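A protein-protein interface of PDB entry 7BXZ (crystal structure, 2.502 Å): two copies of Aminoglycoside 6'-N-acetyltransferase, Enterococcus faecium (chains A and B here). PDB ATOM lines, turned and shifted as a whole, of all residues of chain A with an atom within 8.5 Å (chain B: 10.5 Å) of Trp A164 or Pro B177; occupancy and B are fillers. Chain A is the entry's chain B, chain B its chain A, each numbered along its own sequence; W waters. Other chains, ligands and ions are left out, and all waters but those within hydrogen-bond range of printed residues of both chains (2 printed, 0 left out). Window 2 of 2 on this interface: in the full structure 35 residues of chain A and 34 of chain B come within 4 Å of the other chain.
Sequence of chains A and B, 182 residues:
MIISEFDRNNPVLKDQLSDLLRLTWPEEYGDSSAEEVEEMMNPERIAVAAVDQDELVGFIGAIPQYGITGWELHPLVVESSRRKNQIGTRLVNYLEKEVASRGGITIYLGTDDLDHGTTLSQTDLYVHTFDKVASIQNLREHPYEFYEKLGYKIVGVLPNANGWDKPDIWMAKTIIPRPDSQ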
ATOM      1  N   ASP A 113      13.035  28.432  37.073  1.00  0.00           N
ATOM      2  CA  ASP A 113      11.593  28.435  37.317  1.00  0.00           C
ATOM      3  C   ASP A 113      10.990  27.255  36.560  1.00  0.00           C
ATOM      4  O   ASP A 113      10.685  27.354  35.369  1.00  0.00           O
ATOM      5  CB  ASP A 113      10.948  29.749  36.900  1.00  0.00           C
ATOM      6  CG  ASP A 113       9.539  29.892  37.443  1.00  0.00           C
ATOM      7  OD1 ASP A 113       9.044  28.937  38.084  1.00  0.00           O
ATOM      8  OD2 ASP A 113       8.924  30.959  37.233  1.00  0.00           O
ATOM      9  N   LEU A 114      10.813  26.135  37.260  1.00  0.00           N
ATOM     10  CA  LEU A 114      10.331  24.923  36.615  1.00  0.00           C
ATOM     11  C   LEU A 114       8.810  24.810  36.604  1.00  0.00           C
ATOM     12  O   LEU A 114       8.253  24.264  35.643  1.00  0.00           O
ATOM     13  CB  LEU A 114      10.934  23.689  37.297  1.00  0.00           C
ATOM     14  CG  LEU A 114      12.459  23.622  37.413  1.00  0.00           C
ATOM     15  CD1 LEU A 114      12.900  22.264  37.936  1.00  0.00           C
ATOM     16  CD2 LEU A 114      13.101  23.910  36.070  1.00  0.00           C
ATOM     17  N   LEU A 120       7.723  34.775  34.910  1.00  0.00           N
ATOM     18  CA  LEU A 120       8.582  34.569  33.749  1.00  0.00           C
ATOM     19  C   LEU A 120       8.414  33.185  33.137  1.00  0.00           C
ATOM     20  O   LEU A 120       8.834  32.971  31.994  1.00  0.00           O
ATOM     21  CB  LEU A 120      10.049  34.793  34.126  1.00  0.00           C
ATOM     22  CG  LEU A 120      10.432  36.208  34.565  1.00  0.00           C
ATOM     23  CD1 LEU A 120      11.937  36.332  34.765  1.00  0.00           C
ATOM     24  CD2 LEU A 120       9.940  37.232  33.557  1.00  0.00           C
ATOM     25  N   SER A 121       7.835  32.244  33.876  1.00  0.00           N
ATOM     26  CA  SER A 121       7.479  30.935  33.357  1.00  0.00           C
ATOM     27  C   SER A 121       6.075  30.957  32.756  1.00  0.00           C
ATOM     28  O   SER A 121       5.329  31.930  32.888  1.00  0.00           O
ATOM     29  CB  SER A 121       7.563  29.886  34.461  1.00  0.00           C
ATOM     30  OG  SER A 121       6.740  30.266  35.543  1.00  0.00           O
ATOM     31  N   GLN A 122       5.722  29.855  32.090  1.00  0.00           N
ATOM     32  CA  GLN A 122       4.417  29.690  31.446  1.00  0.00           C
ATOM     33  C   GLN A 122       4.118  30.843  30.493  1.00  0.00           C
ATOM     34  O   GLN A 122       2.985  31.316  30.388  1.00  0.00           O
ATOM     35  CB  GLN A 122       3.303  29.549  32.486  1.00  0.00           C
ATOM     36  CG  GLN A 122       3.247  28.198  33.173  1.00  0.00           C
ATOM     37  CD  GLN A 122       1.973  28.009  33.973  1.00  0.00           C
ATOM     38  NE2 GLN A 122       1.921  26.939  34.760  1.00  0.00           N
ATOM     39  N   THR A 123       5.150  31.294  29.785  1.00  0.00           N
ATOM     40  CA  THR A 123       4.995  32.321  28.768  1.00  0.00           C
ATOM     41  C   THR A 123       6.171  32.226  27.808  1.00  0.00           C
ATOM     42  O   THR A 123       7.233  31.700  28.152  1.00  0.00           O
ATOM     43  CB  THR A 123       4.922  33.723  29.383  1.00  0.00           C
ATOM     44  OG1 THR A 123       4.935  34.709  28.341  1.00  0.00           O
ATOM     45  CG2 THR A 123       6.109  33.960  30.305  1.00  0.00           C
ATOM     46  N   ASP A 124       5.977  32.765  26.610  1.00  0.00           N
ATOM     47  CA  ASP A 124       7.044  32.796  25.617  1.00  0.00           C
ATOM     48  C   ASP A 124       7.940  33.975  25.968  1.00  0.00           C
ATOM     49  O   ASP A 124       7.613  35.130  25.682  1.00  0.00           O
ATOM     50  CB  ASP A 124       6.476  32.915  24.206  1.00  0.00           C
ATOM     51  CG  ASP A 124       7.547  32.806  23.127  1.00  0.00           C
ATOM     52  OD1 ASP A 124       8.752  32.837  23.456  1.00  0.00           O
ATOM     53  OD2 ASP A 124       7.180  32.684  21.940  1.00  0.00           O
ATOM     54  N   LEU A 125       9.084  33.682  26.590  1.00  0.00           N
ATOM     55  CA  LEU A 125       9.976  34.736  27.052  1.00  0.00           C
ATOM     56  C   LEU A 125      10.656  35.469  25.908  1.00  0.00           C
ATOM     57  O   LEU A 125      11.318  36.481  26.153  1.00  0.00           O
ATOM     58  CB  LEU A 125      11.036  34.160  27.993  1.00  0.00           C
ATOM     59  CG  LEU A 125      10.790  34.313  29.495  1.00  0.00           C
ATOM     60  CD1 LEU A 125      11.982  33.798  30.286  1.00  0.00           C
ATOM     61  CD2 LEU A 125      10.501  35.763  29.846  1.00  0.00           C
ATOM     62  N   TYR A 126      10.520  34.985  24.676  1.00  0.00           N
ATOM     63  CA  TYR A 126      11.019  35.717  23.522  1.00  0.00           C
ATOM     64  C   TYR A 126      10.092  36.849  23.095  1.00  0.00           C
ATOM     65  O   TYR A 126      10.474  37.650  22.234  1.00  0.00           O
ATOM     66  CB  TYR A 126      11.270  34.749  22.365  1.00  0.00           C
ATOM     67  CG  TYR A 126      12.602  34.052  22.504  1.00  0.00           C
ATOM     68  CD1 TYR A 126      13.786  34.761  22.366  1.00  0.00           C
ATOM     69  CD2 TYR A 126      12.680  32.697  22.808  1.00  0.00           C
ATOM     70  CE1 TYR A 126      15.009  34.144  22.506  1.00  0.00           C
ATOM     71  CE2 TYR A 126      13.903  32.068  22.949  1.00  0.00           C
ATOM     72  CZ  TYR A 126      15.064  32.799  22.797  1.00  0.00           C
ATOM     73  OH  TYR A 126      16.289  32.191  22.935  1.00  0.00           O
ATOM     74  N   LEU A 158      17.233  32.798  30.510  1.00  0.00           N
ATOM     75  CA  LEU A 158      17.422  31.862  29.406  1.00  0.00           C
ATOM     76  C   LEU A 158      16.087  31.222  29.054  1.00  0.00           C
ATOM     77  O   LEU A 158      15.631  30.309  29.761  1.00  0.00           O
ATOM     78  CB  LEU A 158      18.457  30.791  29.762  1.00  0.00           C
ATOM     79  CG  LEU A 158      18.677  29.689  28.720  1.00  0.00           C
ATOM     80  CD1 LEU A 158      18.852  30.265  27.328  1.00  0.00           C
ATOM     81  CD2 LEU A 158      19.882  28.847  29.091  1.00  0.00           C
ATOM     82  N   PRO A 159      15.416  31.673  27.995  1.00  0.00           N
ATOM     83  CA  PRO A 159      14.094  31.126  27.669  1.00  0.00           C
ATOM     84  C   PRO A 159      14.170  29.647  27.313  1.00  0.00           C
ATOM     85  O   PRO A 159      15.083  29.202  26.612  1.00  0.00           O
ATOM     86  CB  PRO A 159      13.647  31.970  26.471  1.00  0.00           C
ATOM     87  CG  PRO A 159      14.470  33.215  26.545  1.00  0.00           C
ATOM     88  CD  PRO A 159      15.790  32.784  27.106  1.00  0.00           C
ATOM     89  N   ASN A 160      13.200  28.886  27.824  1.00  0.00           N
ATOM     90  CA  ASN A 160      13.048  27.461  27.522  1.00  0.00           C
ATOM     91  C   ASN A 160      14.272  26.649  27.937  1.00  0.00           C
ATOM     92  O   ASN A 160      14.590  25.633  27.313  1.00  0.00           O
ATOM     93  CB  ASN A 160      12.746  27.229  26.038  1.00  0.00           C
ATOM     94  CG  ASN A 160      11.738  28.212  25.483  1.00  0.00           C
ATOM     95  OD1 ASN A 160      10.636  28.359  26.015  1.00  0.00           O
ATOM     96  ND2 ASN A 160      12.109  28.890  24.404  1.00  0.00           N
ATOM     97  N   ALA A 161      14.958  27.082  28.998  1.00  0.00           N
ATOM     98  CA  ALA A 161      16.188  26.415  29.418  1.00  0.00           C
ATOM     99  C   ALA A 161      15.930  24.968  29.823  1.00  0.00           C
ATOM    100  O   ALA A 161      16.620  24.051  29.364  1.00  0.00           O
ATOM    101  CB  ALA A 161      16.833  27.187  30.569  1.00  0.00           C
ATOM    102  N   ASN A 162      14.928  24.742  30.673  1.00  0.00           N
ATOM    103  CA  ASN A 162      14.642  23.428  31.235  1.00  0.00           C
ATOM    104  C   ASN A 162      13.455  22.756  30.559  1.00  0.00           C
ATOM    105  O   ASN A 162      12.808  21.893  31.160  1.00  0.00           O
ATOM    106  CB  ASN A 162      14.386  23.549  32.737  1.00  0.00           C
ATOM    107  CG  ASN A 162      15.485  24.304  33.456  1.00  0.00           C
ATOM    108  OD1 ASN A 162      16.541  23.748  33.754  1.00  0.00           O
ATOM    109  ND2 ASN A 162      15.246  25.583  33.728  1.00  0.00           N
ATOM    110  N   GLY A 163      13.165  23.127  29.323  1.00  0.00           N
ATOM    111  CA  GLY A 163      11.908  22.807  28.683  1.00  0.00           C
ATOM    112  C   GLY A 163      11.143  24.069  28.333  1.00  0.00           C
ATOM    113  O   GLY A 163      11.464  25.171  28.774  1.00  0.00           O
ATOM    114  N   TRP A 164      10.102  23.878  27.528  1.00  0.00           N
ATOM    115  CA  TRP A 164       9.331  25.010  27.030  1.00  0.00           C
ATOM    116  C   TRP A 164       8.757  25.824  28.180  1.00  0.00           C
ATOM    117  O   TRP A 164       8.054  25.289  29.045  1.00  0.00           O
ATOM    118  CB  TRP A 164       8.223  24.514  26.103  1.00  0.00           C
ATOM    119  CG  TRP A 164       8.758  24.130  24.765  1.00  0.00           C
ATOM    120  CD1 TRP A 164       8.932  22.869  24.282  1.00  0.00           C
ATOM    121  CD2 TRP A 164       9.234  25.019  23.750  1.00  0.00           C
ATOM    122  NE1 TRP A 164       9.471  22.917  23.019  1.00  0.00           N
ATOM    123  CE2 TRP A 164       9.666  24.227  22.669  1.00  0.00           C
ATOM    124  CE3 TRP A 164       9.329  26.412  23.647  1.00  0.00           C
ATOM    125  CZ2 TRP A 164      10.182  24.776  21.500  1.00  0.00           C
ATOM    126  CZ3 TRP A 164       9.842  26.956  22.484  1.00  0.00           C
ATOM    127  CH2 TRP A 164      10.260  26.138  21.427  1.00  0.00           C
ATOM    128  N   ASP A 165       9.079  27.121  28.185  1.00  0.00           N
ATOM    129  CA  ASP A 165       8.573  28.068  29.176  1.00  0.00           C
ATOM    130  C   ASP A 165       8.959  27.677  30.600  1.00  0.00           C
ATOM    131  O   ASP A 165       8.247  27.976  31.557  1.00  0.00           O
ATOM    132  CB  ASP A 165       7.059  28.257  29.035  1.00  0.00           C
ATOM    133  CG  ASP A 165       6.660  28.642  27.625  1.00  0.00           C
ATOM    134  OD1 ASP A 165       7.500  29.249  26.921  1.00  0.00           O
ATOM    135  OD2 ASP A 165       5.509  28.382  27.216  1.00  0.00           O
ATOM    136  N   LYS A 166      10.101  27.012  30.742  1.00  0.00           N
ATOM    137  CA  LYS A 166      10.690  26.682  32.040  1.00  0.00           C
ATOM    138  C   LYS A 166      12.090  27.277  32.017  1.00  0.00           C
ATOM    139  O   LYS A 166      13.079  26.564  31.800  1.00  0.00           O
ATOM    140  CB  LYS A 166      10.710  25.173  32.276  1.00  0.00           C
ATOM    141  CG  LYS A 166       9.336  24.539  32.337  1.00  0.00           C
ATOM    142  CD  LYS A 166       9.418  23.075  32.729  1.00  0.00           C
ATOM    143  CE  LYS A 166       8.075  22.386  32.533  1.00  0.00           C
ATOM    144  NZ  LYS A 166       7.028  23.030  33.373  1.00  0.00           N
ATOM    145  N   PRO A 167      12.209  28.581  32.229  1.00  0.00           N
ATOM    146  CA  PRO A 167      13.495  29.250  32.033  1.00  0.00           C
ATOM    147  C   PRO A 167      14.382  29.281  33.269  1.00  0.00           C
ATOM    148  O   PRO A 167      13.975  28.927  34.375  1.00  0.00           O
ATOM    149  CB  PRO A 167      13.053  30.669  31.657  1.00  0.00           C
ATOM    150  CG  PRO A 167      11.862  30.889  32.548  1.00  0.00           C
ATOM    151  CD  PRO A 167      11.162  29.534  32.641  1.00  0.00           C
ATOM    152  N   TYR B  66      21.347  22.018  30.593  1.00  0.00           N
ATOM    153  CA  TYR B  66      20.015  21.828  31.164  1.00  0.00           C
ATOM    154  C   TYR B  66      19.427  20.548  30.580  1.00  0.00           C
ATOM    155  O   TYR B  66      18.785  20.584  29.525  1.00  0.00           O
ATOM    156  CB  TYR B  66      19.112  23.015  30.884  1.00  0.00           C
ATOM    157  CG  TYR B  66      19.635  24.337  31.383  1.00  0.00           C
ATOM    158  CD1 TYR B  66      20.540  25.073  30.632  1.00  0.00           C
ATOM    159  CD2 TYR B  66      19.213  24.858  32.598  1.00  0.00           C
ATOM    160  CE1 TYR B  66      21.018  26.283  31.081  1.00  0.00           C
ATOM    161  CE2 TYR B  66      19.684  26.072  33.055  1.00  0.00           C
ATOM    162  CZ  TYR B  66      20.585  26.781  32.290  1.00  0.00           C
ATOM    163  OH  TYR B  66      21.060  27.990  32.735  1.00  0.00           O
ATOM    164  N   ILE B  68      18.568  17.683  28.510  1.00  0.00           N
ATOM    165  CA  ILE B  68      18.764  17.641  27.068  1.00  0.00           C
ATOM    166  C   ILE B  68      18.161  18.845  26.374  1.00  0.00           C
ATOM    167  O   ILE B  68      18.258  18.949  25.143  1.00  0.00           O
ATOM    168  CB  ILE B  68      18.196  16.343  26.462  1.00  0.00           C
ATOM    169  CG1 ILE B  68      16.668  16.337  26.560  1.00  0.00           C
ATOM    170  CG2 ILE B  68      18.782  15.127  27.160  1.00  0.00           C
ATOM    171  CD1 ILE B  68      16.004  15.252  25.743  1.00  0.00           C
ATOM    172  N   THR B  69      17.549  19.767  27.118  1.00  0.00           N
ATOM    173  CA  THR B  69      16.863  20.896  26.503  1.00  0.00           C
ATOM    174  C   THR B  69      17.779  22.090  26.263  1.00  0.00           C
ATOM    175  O   THR B  69      17.680  22.739  25.217  1.00  0.00           O
ATOM    176  CB  THR B  69      15.677  21.331  27.369  1.00  0.00           C
ATOM    177  OG1 THR B  69      16.127  21.599  28.700  1.00  0.00           O
ATOM    178  CG2 THR B  69      14.617  20.239  27.407  1.00  0.00           C
ATOM    179  N   GLY B  70      18.674  22.392  27.203  1.00  0.00           N
ATOM    180  CA  GLY B  70      19.516  23.567  27.060  1.00  0.00           C
ATOM    181  C   GLY B  70      20.993  23.288  26.878  1.00  0.00           C
ATOM    182  O   GLY B  70      21.623  22.694  27.762  1.00  0.00           O
ATOM    183  N   GLU B  96      23.257  23.327  15.460  1.00  0.00           N
ATOM    184  CA  GLU B  96      21.840  23.485  15.774  1.00  0.00           C
ATOM    185  C   GLU B  96      21.051  22.250  15.365  1.00  0.00           C
ATOM    186  O   GLU B  96      20.183  21.779  16.111  1.00  0.00           O
ATOM    187  CB  GLU B  96      21.277  24.724  15.078  1.00  0.00           C
ATOM    188  CG  GLU B  96      21.855  26.040  15.556  1.00  0.00           C
ATOM    189  CD  GLU B  96      21.175  27.235  14.921  1.00  0.00           C
ATOM    190  OE1 GLU B  96      20.151  27.040  14.232  1.00  0.00           O
ATOM    191  OE2 GLU B  96      21.666  28.370  15.106  1.00  0.00           O
ATOM    192  N   ALA B 100      19.005  19.828  17.950  1.00  0.00           N
ATOM    193  CA  ALA B 100      17.601  19.504  17.716  1.00  0.00           C
ATOM    194  C   ALA B 100      17.394  17.997  17.623  1.00  0.00           C
ATOM    195  O   ALA B 100      16.404  17.464  18.142  1.00  0.00           O
ATOM    196  CB  ALA B 100      17.105  20.196  16.448  1.00  0.00           C
ATOM    197  N   SER B 101      18.315  17.295  16.956  1.00  0.00           N
ATOM    198  CA  SER B 101      18.193  15.850  16.791  1.00  0.00           C
ATOM    199  C   SER B 101      18.137  15.111  18.122  1.00  0.00           C
ATOM    200  O   SER B 101      17.478  14.070  18.221  1.00  0.00           O
ATOM    201  CB  SER B 101      19.362  15.326  15.954  1.00  0.00           C
ATOM    202  OG  SER B 101      20.449  14.950  16.789  1.00  0.00           O
ATOM    203  N   GLY B 103      16.753  16.177  20.891  1.00  0.00           N
ATOM    204  CA  GLY B 103      15.701  16.708  21.735  1.00  0.00           C
ATOM    205  C   GLY B 103      15.987  18.067  22.330  1.00  0.00           C
ATOM    206  O   GLY B 103      15.304  18.471  23.276  1.00  0.00           O
ATOM    207  N   GLY B 104      16.984  18.781  21.811  1.00  0.00           N
ATOM    208  CA  GLY B 104      17.326  20.088  22.342  1.00  0.00           C
ATOM    209  C   GLY B 104      16.381  21.181  21.876  1.00  0.00           C
ATOM    210  O   GLY B 104      15.798  21.122  20.791  1.00  0.00           O
ATOM    211  N   ILE B 105      16.224  22.195  22.725  1.00  0.00           N
ATOM    212  CA  ILE B 105      15.354  23.332  22.444  1.00  0.00           C
ATOM    213  C   ILE B 105      16.159  24.592  22.160  1.00  0.00           C
ATOM    214  O   ILE B 105      15.944  25.260  21.148  1.00  0.00           O
ATOM    215  CB  ILE B 105      14.360  23.577  23.601  1.00  0.00           C
ATOM    216  CG1 ILE B 105      13.538  22.327  23.907  1.00  0.00           C
ATOM    217  CG2 ILE B 105      13.447  24.746  23.283  1.00  0.00           C
ATOM    218  CD1 ILE B 105      12.739  22.442  25.187  1.00  0.00           C
ATOM    219  N   THR B 106      17.115  24.914  23.030  1.00  0.00           N
ATOM    220  CA  THR B 106      17.832  26.175  22.922  1.00  0.00           C
ATOM    221  C   THR B 106      19.337  25.998  23.069  1.00  0.00           C
ATOM    222  O   THR B 106      19.811  25.154  23.840  1.00  0.00           O
ATOM    223  CB  THR B 106      17.337  27.179  23.969  1.00  0.00           C
ATOM    224  OG1 THR B 106      18.201  28.323  23.982  1.00  0.00           O
ATOM    225  CG2 THR B 106      17.323  26.547  25.350  1.00  0.00           C
ATOM    226  N   ILE B 107      20.070  26.805  22.304  1.00  0.00           N
ATOM    227  CA  ILE B 107      21.519  26.927  22.400  1.00  0.00           C
ATOM    228  C   ILE B 107      21.826  28.340  22.878  1.00  0.00           C
ATOM    229  O   ILE B 107      21.307  29.315  22.323  1.00  0.00           O
ATOM    230  CB  ILE B 107      22.205  26.643  21.052  1.00  0.00           C
ATOM    231  CG1 ILE B 107      22.015  25.181  20.641  1.00  0.00           C
ATOM    232  CG2 ILE B 107      23.686  26.992  21.118  1.00  0.00           C
ATOM    233  CD1 ILE B 107      22.720  24.829  19.349  1.00  0.00           C
ATOM    234  N   LYS B 173      19.233  31.163  21.532  1.00  0.00           N
ATOM    235  CA  LYS B 173      18.357  30.942  20.393  1.00  0.00           C
ATOM    236  C   LYS B 173      17.650  29.611  20.570  1.00  0.00           C
ATOM    237  O   LYS B 173      18.295  28.590  20.835  1.00  0.00           O
ATOM    238  CB  LYS B 173      19.131  30.950  19.072  1.00  0.00           C
ATOM    239  CG  LYS B 173      18.378  30.311  17.917  1.00  0.00           C
ATOM    240  CD  LYS B 173      19.149  30.431  16.616  1.00  0.00           C
ATOM    241  CE  LYS B 173      18.348  29.880  15.449  1.00  0.00           C
ATOM    242  NZ  LYS B 173      19.161  29.819  14.204  1.00  0.00           N
ATOM    243  N   THR B 174      16.331  29.628  20.422  1.00  0.00           N
ATOM    244  CA  THR B 174      15.533  28.413  20.443  1.00  0.00           C
ATOM    245  C   THR B 174      15.468  27.872  19.020  1.00  0.00           C
ATOM    246  O   THR B 174      15.026  28.574  18.104  1.00  0.00           O
ATOM    247  CB  THR B 174      14.140  28.694  21.002  1.00  0.00           C
ATOM    248  OG1 THR B 174      14.202  28.740  22.435  1.00  0.00           O
ATOM    249  CG2 THR B 174      13.173  27.614  20.577  1.00  0.00           C
ATOM    250  N   ILE B 175      15.918  26.630  18.838  1.00  0.00           N
ATOM    251  CA  ILE B 175      16.238  26.100  17.517  1.00  0.00           C
ATOM    252  C   ILE B 175      15.174  25.137  16.997  1.00  0.00           C
ATOM    253  O   ILE B 175      15.375  24.514  15.950  1.00  0.00           O
ATOM    254  CB  ILE B 175      17.619  25.432  17.525  1.00  0.00           C
ATOM    255  CG1 ILE B 175      17.595  24.190  18.413  1.00  0.00           C
ATOM    256  CG2 ILE B 175      18.677  26.411  18.009  1.00  0.00           C
ATOM    257  CD1 ILE B 175      18.903  23.471  18.457  1.00  0.00           C
ATOM    258  N   ILE B 176      14.059  24.986  17.703  1.00  0.00           N
ATOM    259  CA  ILE B 176      12.964  24.147  17.221  1.00  0.00           C
ATOM    260  C   ILE B 176      11.682  24.965  17.285  1.00  0.00           C
ATOM    261  O   ILE B 176      11.607  25.973  18.007  1.00  0.00           O
ATOM    262  CB  ILE B 176      12.840  22.835  18.034  1.00  0.00           C
ATOM    263  CG1 ILE B 176      12.596  23.125  19.514  1.00  0.00           C
ATOM    264  CG2 ILE B 176      14.073  21.960  17.842  1.00  0.00           C
ATOM    265  CD1 ILE B 176      12.323  21.876  20.337  1.00  0.00           C
ATOM    266  N   PRO B 177      10.656  24.576  16.525  1.00  0.00           N
ATOM    267  CA  PRO B 177       9.420  25.364  16.531  1.00  0.00           C
ATOM    268  C   PRO B 177       8.714  25.274  17.873  1.00  0.00           C
ATOM    269  O   PRO B 177       8.698  24.228  18.527  1.00  0.00           O
ATOM    270  CB  PRO B 177       8.584  24.726  15.414  1.00  0.00           C
ATOM    271  CG  PRO B 177       9.112  23.333  15.307  1.00  0.00           C
ATOM    272  CD  PRO B 177      10.586  23.469  15.553  1.00  0.00           C
ATOM    273  N   ARG B 178       8.129  26.390  18.274  1.00  0.00           N
ATOM    274  CA  ARG B 178       7.324  26.431  19.481  1.00  0.00           C
ATOM    275  C   ARG B 178       6.086  25.561  19.292  1.00  0.00           C
ATOM    276  O   ARG B 178       5.435  25.642  18.242  1.00  0.00           O
ATOM    277  CB  ARG B 178       6.930  27.868  19.807  1.00  0.00           C
ATOM    278  CG  ARG B 178       6.152  28.002  21.090  1.00  0.00           C
ATOM    279  CD  ARG B 178       6.175  29.418  21.610  1.00  0.00           C
ATOM    280  NE  ARG B 178       5.424  29.513  22.854  1.00  0.00           N
ATOM    281  CZ  ARG B 178       5.972  29.446  24.062  1.00  0.00           C
ATOM    282  NH1 ARG B 178       7.277  29.245  24.191  1.00  0.00           N
ATOM    283  NH2 ARG B 178       5.207  29.545  25.138  1.00  0.00           N
ATOM    284  N   PRO B 179       5.737  24.713  20.257  1.00  0.00           N
ATOM    285  CA  PRO B 179       4.537  23.885  20.088  1.00  0.00           C
ATOM    286  C   PRO B 179       3.276  24.734  20.071  1.00  0.00           C
ATOM    287  O   PRO B 179       3.109  25.656  20.873  1.00  0.00           O
ATOM    288  CB  PRO B 179       4.560  22.958  21.313  1.00  0.00           C
ATOM    289  CG  PRO B 179       5.886  23.176  21.985  1.00  0.00           C
ATOM    290  CD  PRO B 179       6.374  24.518  21.570  1.00  0.00           C
ATOM    291  N   ASP B 180       2.394  24.416  19.129  1.00  0.00           N
ATOM    292  CA  ASP B 180       1.102  25.081  19.012  1.00  0.00           C
ATOM    293  C   ASP B 180      -0.016  24.048  18.901  1.00  0.00           C
ATOM    294  O   ASP B 180      -1.018  24.121  19.611  1.00  0.00           O
ATOM    295  CB  ASP B 180       1.083  26.034  17.811  1.00  0.00           C
ATOM    296  CG  ASP B 180       1.600  25.389  16.538  1.00  0.00           C
ATOM    297  OD1 ASP B 180       1.789  24.155  16.517  1.00  0.00           O
ATOM    298  OD2 ASP B 180       1.821  26.123  15.553  1.00  0.00           O
HETATM  299  O   HOH W   1      16.359  29.900  24.257  1.00  0.00           O
HETATM  300  O   HOH W   2       9.653  30.127  22.909  1.00  0.00           O
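OG1 of Thr B174 sits at hydrogen-bond distance from ND2 of Asn A160 (2.9 Å). NE of Arg B178 lies within salt-bridge range of OD2 of Asp A124, 3.7 Å away. The side-chain hydroxyl (OG1) of Thr B69 sits at hydrogen-bond distance from the backbone NH (N) of Gly A163, at 3.4 Å. N of Lys B173 sits at hydrogen-bond distance from OH of Tyr A126. The guanidinium group (NH2) of Arg B178 lies within salt-bridge range of the side-chain carboxylate (OD2) of Asp A165, 2.4 Å away. The side-chain hydroxyl (OG1) of Thr B69 sits at hydrogen-bond distance from the backbone carbonyl oxygen (O) of Ala A161, at 2.6 Å. N of Gly B70 sits at hydrogen-bond distance from O of Ala A161.
N of Gln A122 sits at hydrogen-bond distance from O of Asp A165. OE1 of Glu B96 lies within salt-bridge range of NZ of Lys B173. The backbone carbonyl oxygen (O) of Lys A166 is in hydrogen-bond range of the backbone NH (N) of Ala A161 (3.4 Å). N of Ile B175 lies within hydrogen-bond range of O of Ile B105, at 2.7 Å. N of Thr B106 lies within hydrogen-bond range of O of Thr B69, at 3.1 Å.
Among the printed residues, merely in contact across the chains: Thr A123 with Arg B178, Tyr A126 with Thr B174, Leu A158 with Tyr B66, Leu A158 with Thr B106, Pro A159 with Thr B106, Asn A160 with Ile B105, Asn A160 with Thr B106, Asn A160 with Arg B178, Ala A161 with Tyr B66, Asn A162 with Tyr B66, Asn A162 with Thr B69, Gly A163 with Ile B105, Trp A164 with Ile B105, Trp A164 with Thr B174, Trp A164 with Ile B176, Trp A164 with Pro B177, Trp A164 with Arg B178 and Trp A164 with Pro B179.
Trp A164 touches just these residues of chain B: Ile B105, Thr B174, Ile B176, Pro B177, Arg B178 and Pro B179. Of chain A, only Trp A164 comes within 4 Å of Pro B177. Of chain B, only Ile B105 (3.8 Å), Thr B106 (3.5 Å), Thr B174 (2.9 Å) and Arg B178 (3.9 Å) come within 4 Å of Asn A160. Gly A163 touches two residues of chain B. Of chain B, only Arg B178 comes within 4 Å of Asp A165. Lys A166 touches none of the printed residues of chain B. Of chain A, only Trp A164 comes within 4 Å of Ile B176. Printed residues of chain A within 4 Å of Tyr B66: Leu A158 (3.4 Å), Ala A161 (3.1 Å) and Asn A162 (3.1 Å). Of the printed residues of chain B, Asp A124 touches Arg B178. Of the printed residues of chain A, Thr B174 touches Tyr A126 (3.4 Å), Asn A160 (2.9 Å) and Trp A164 (3.4 Å). The nearest residue of chain B that does not touch Trp A164 is Thr B69 (5.8 Å). The nearest residue of chain A that does not touch Pro B177 is Asn A160 (8.2 Å). The nearest printed residue of chain B that does not touch Asp A124 is Thr B174 (6.9 Å).
Of the 20 printed residues of chain B, 11 touch a printed residue of chain A. Of the 19 printed residues of chain A, 11 touch a printed residue of chain B. Among the printed residues, Asp or Glu carboxylates within 4 Å of a Lys or Arg side-chain nitrogen of the other chain: Asp A124 with Arg B178 (3.7 Å) and Asp A165 with Arg B178 (2.4 Å).
No position is printed for both chains.
Water W1 lies within hydrogen-bond range of OG1 of Thr B106, OH of Tyr A126, O of Pro A159 and OG1 of Thr B174. Water W2 lies within hydrogen-bond range of the guanidinium group of Arg B178 (2.8 Å), the side-chain carboxylate of Asp A124 (2.9 Å) and the side-chain amide nitrogen of Asn A160 (3.1 Å).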
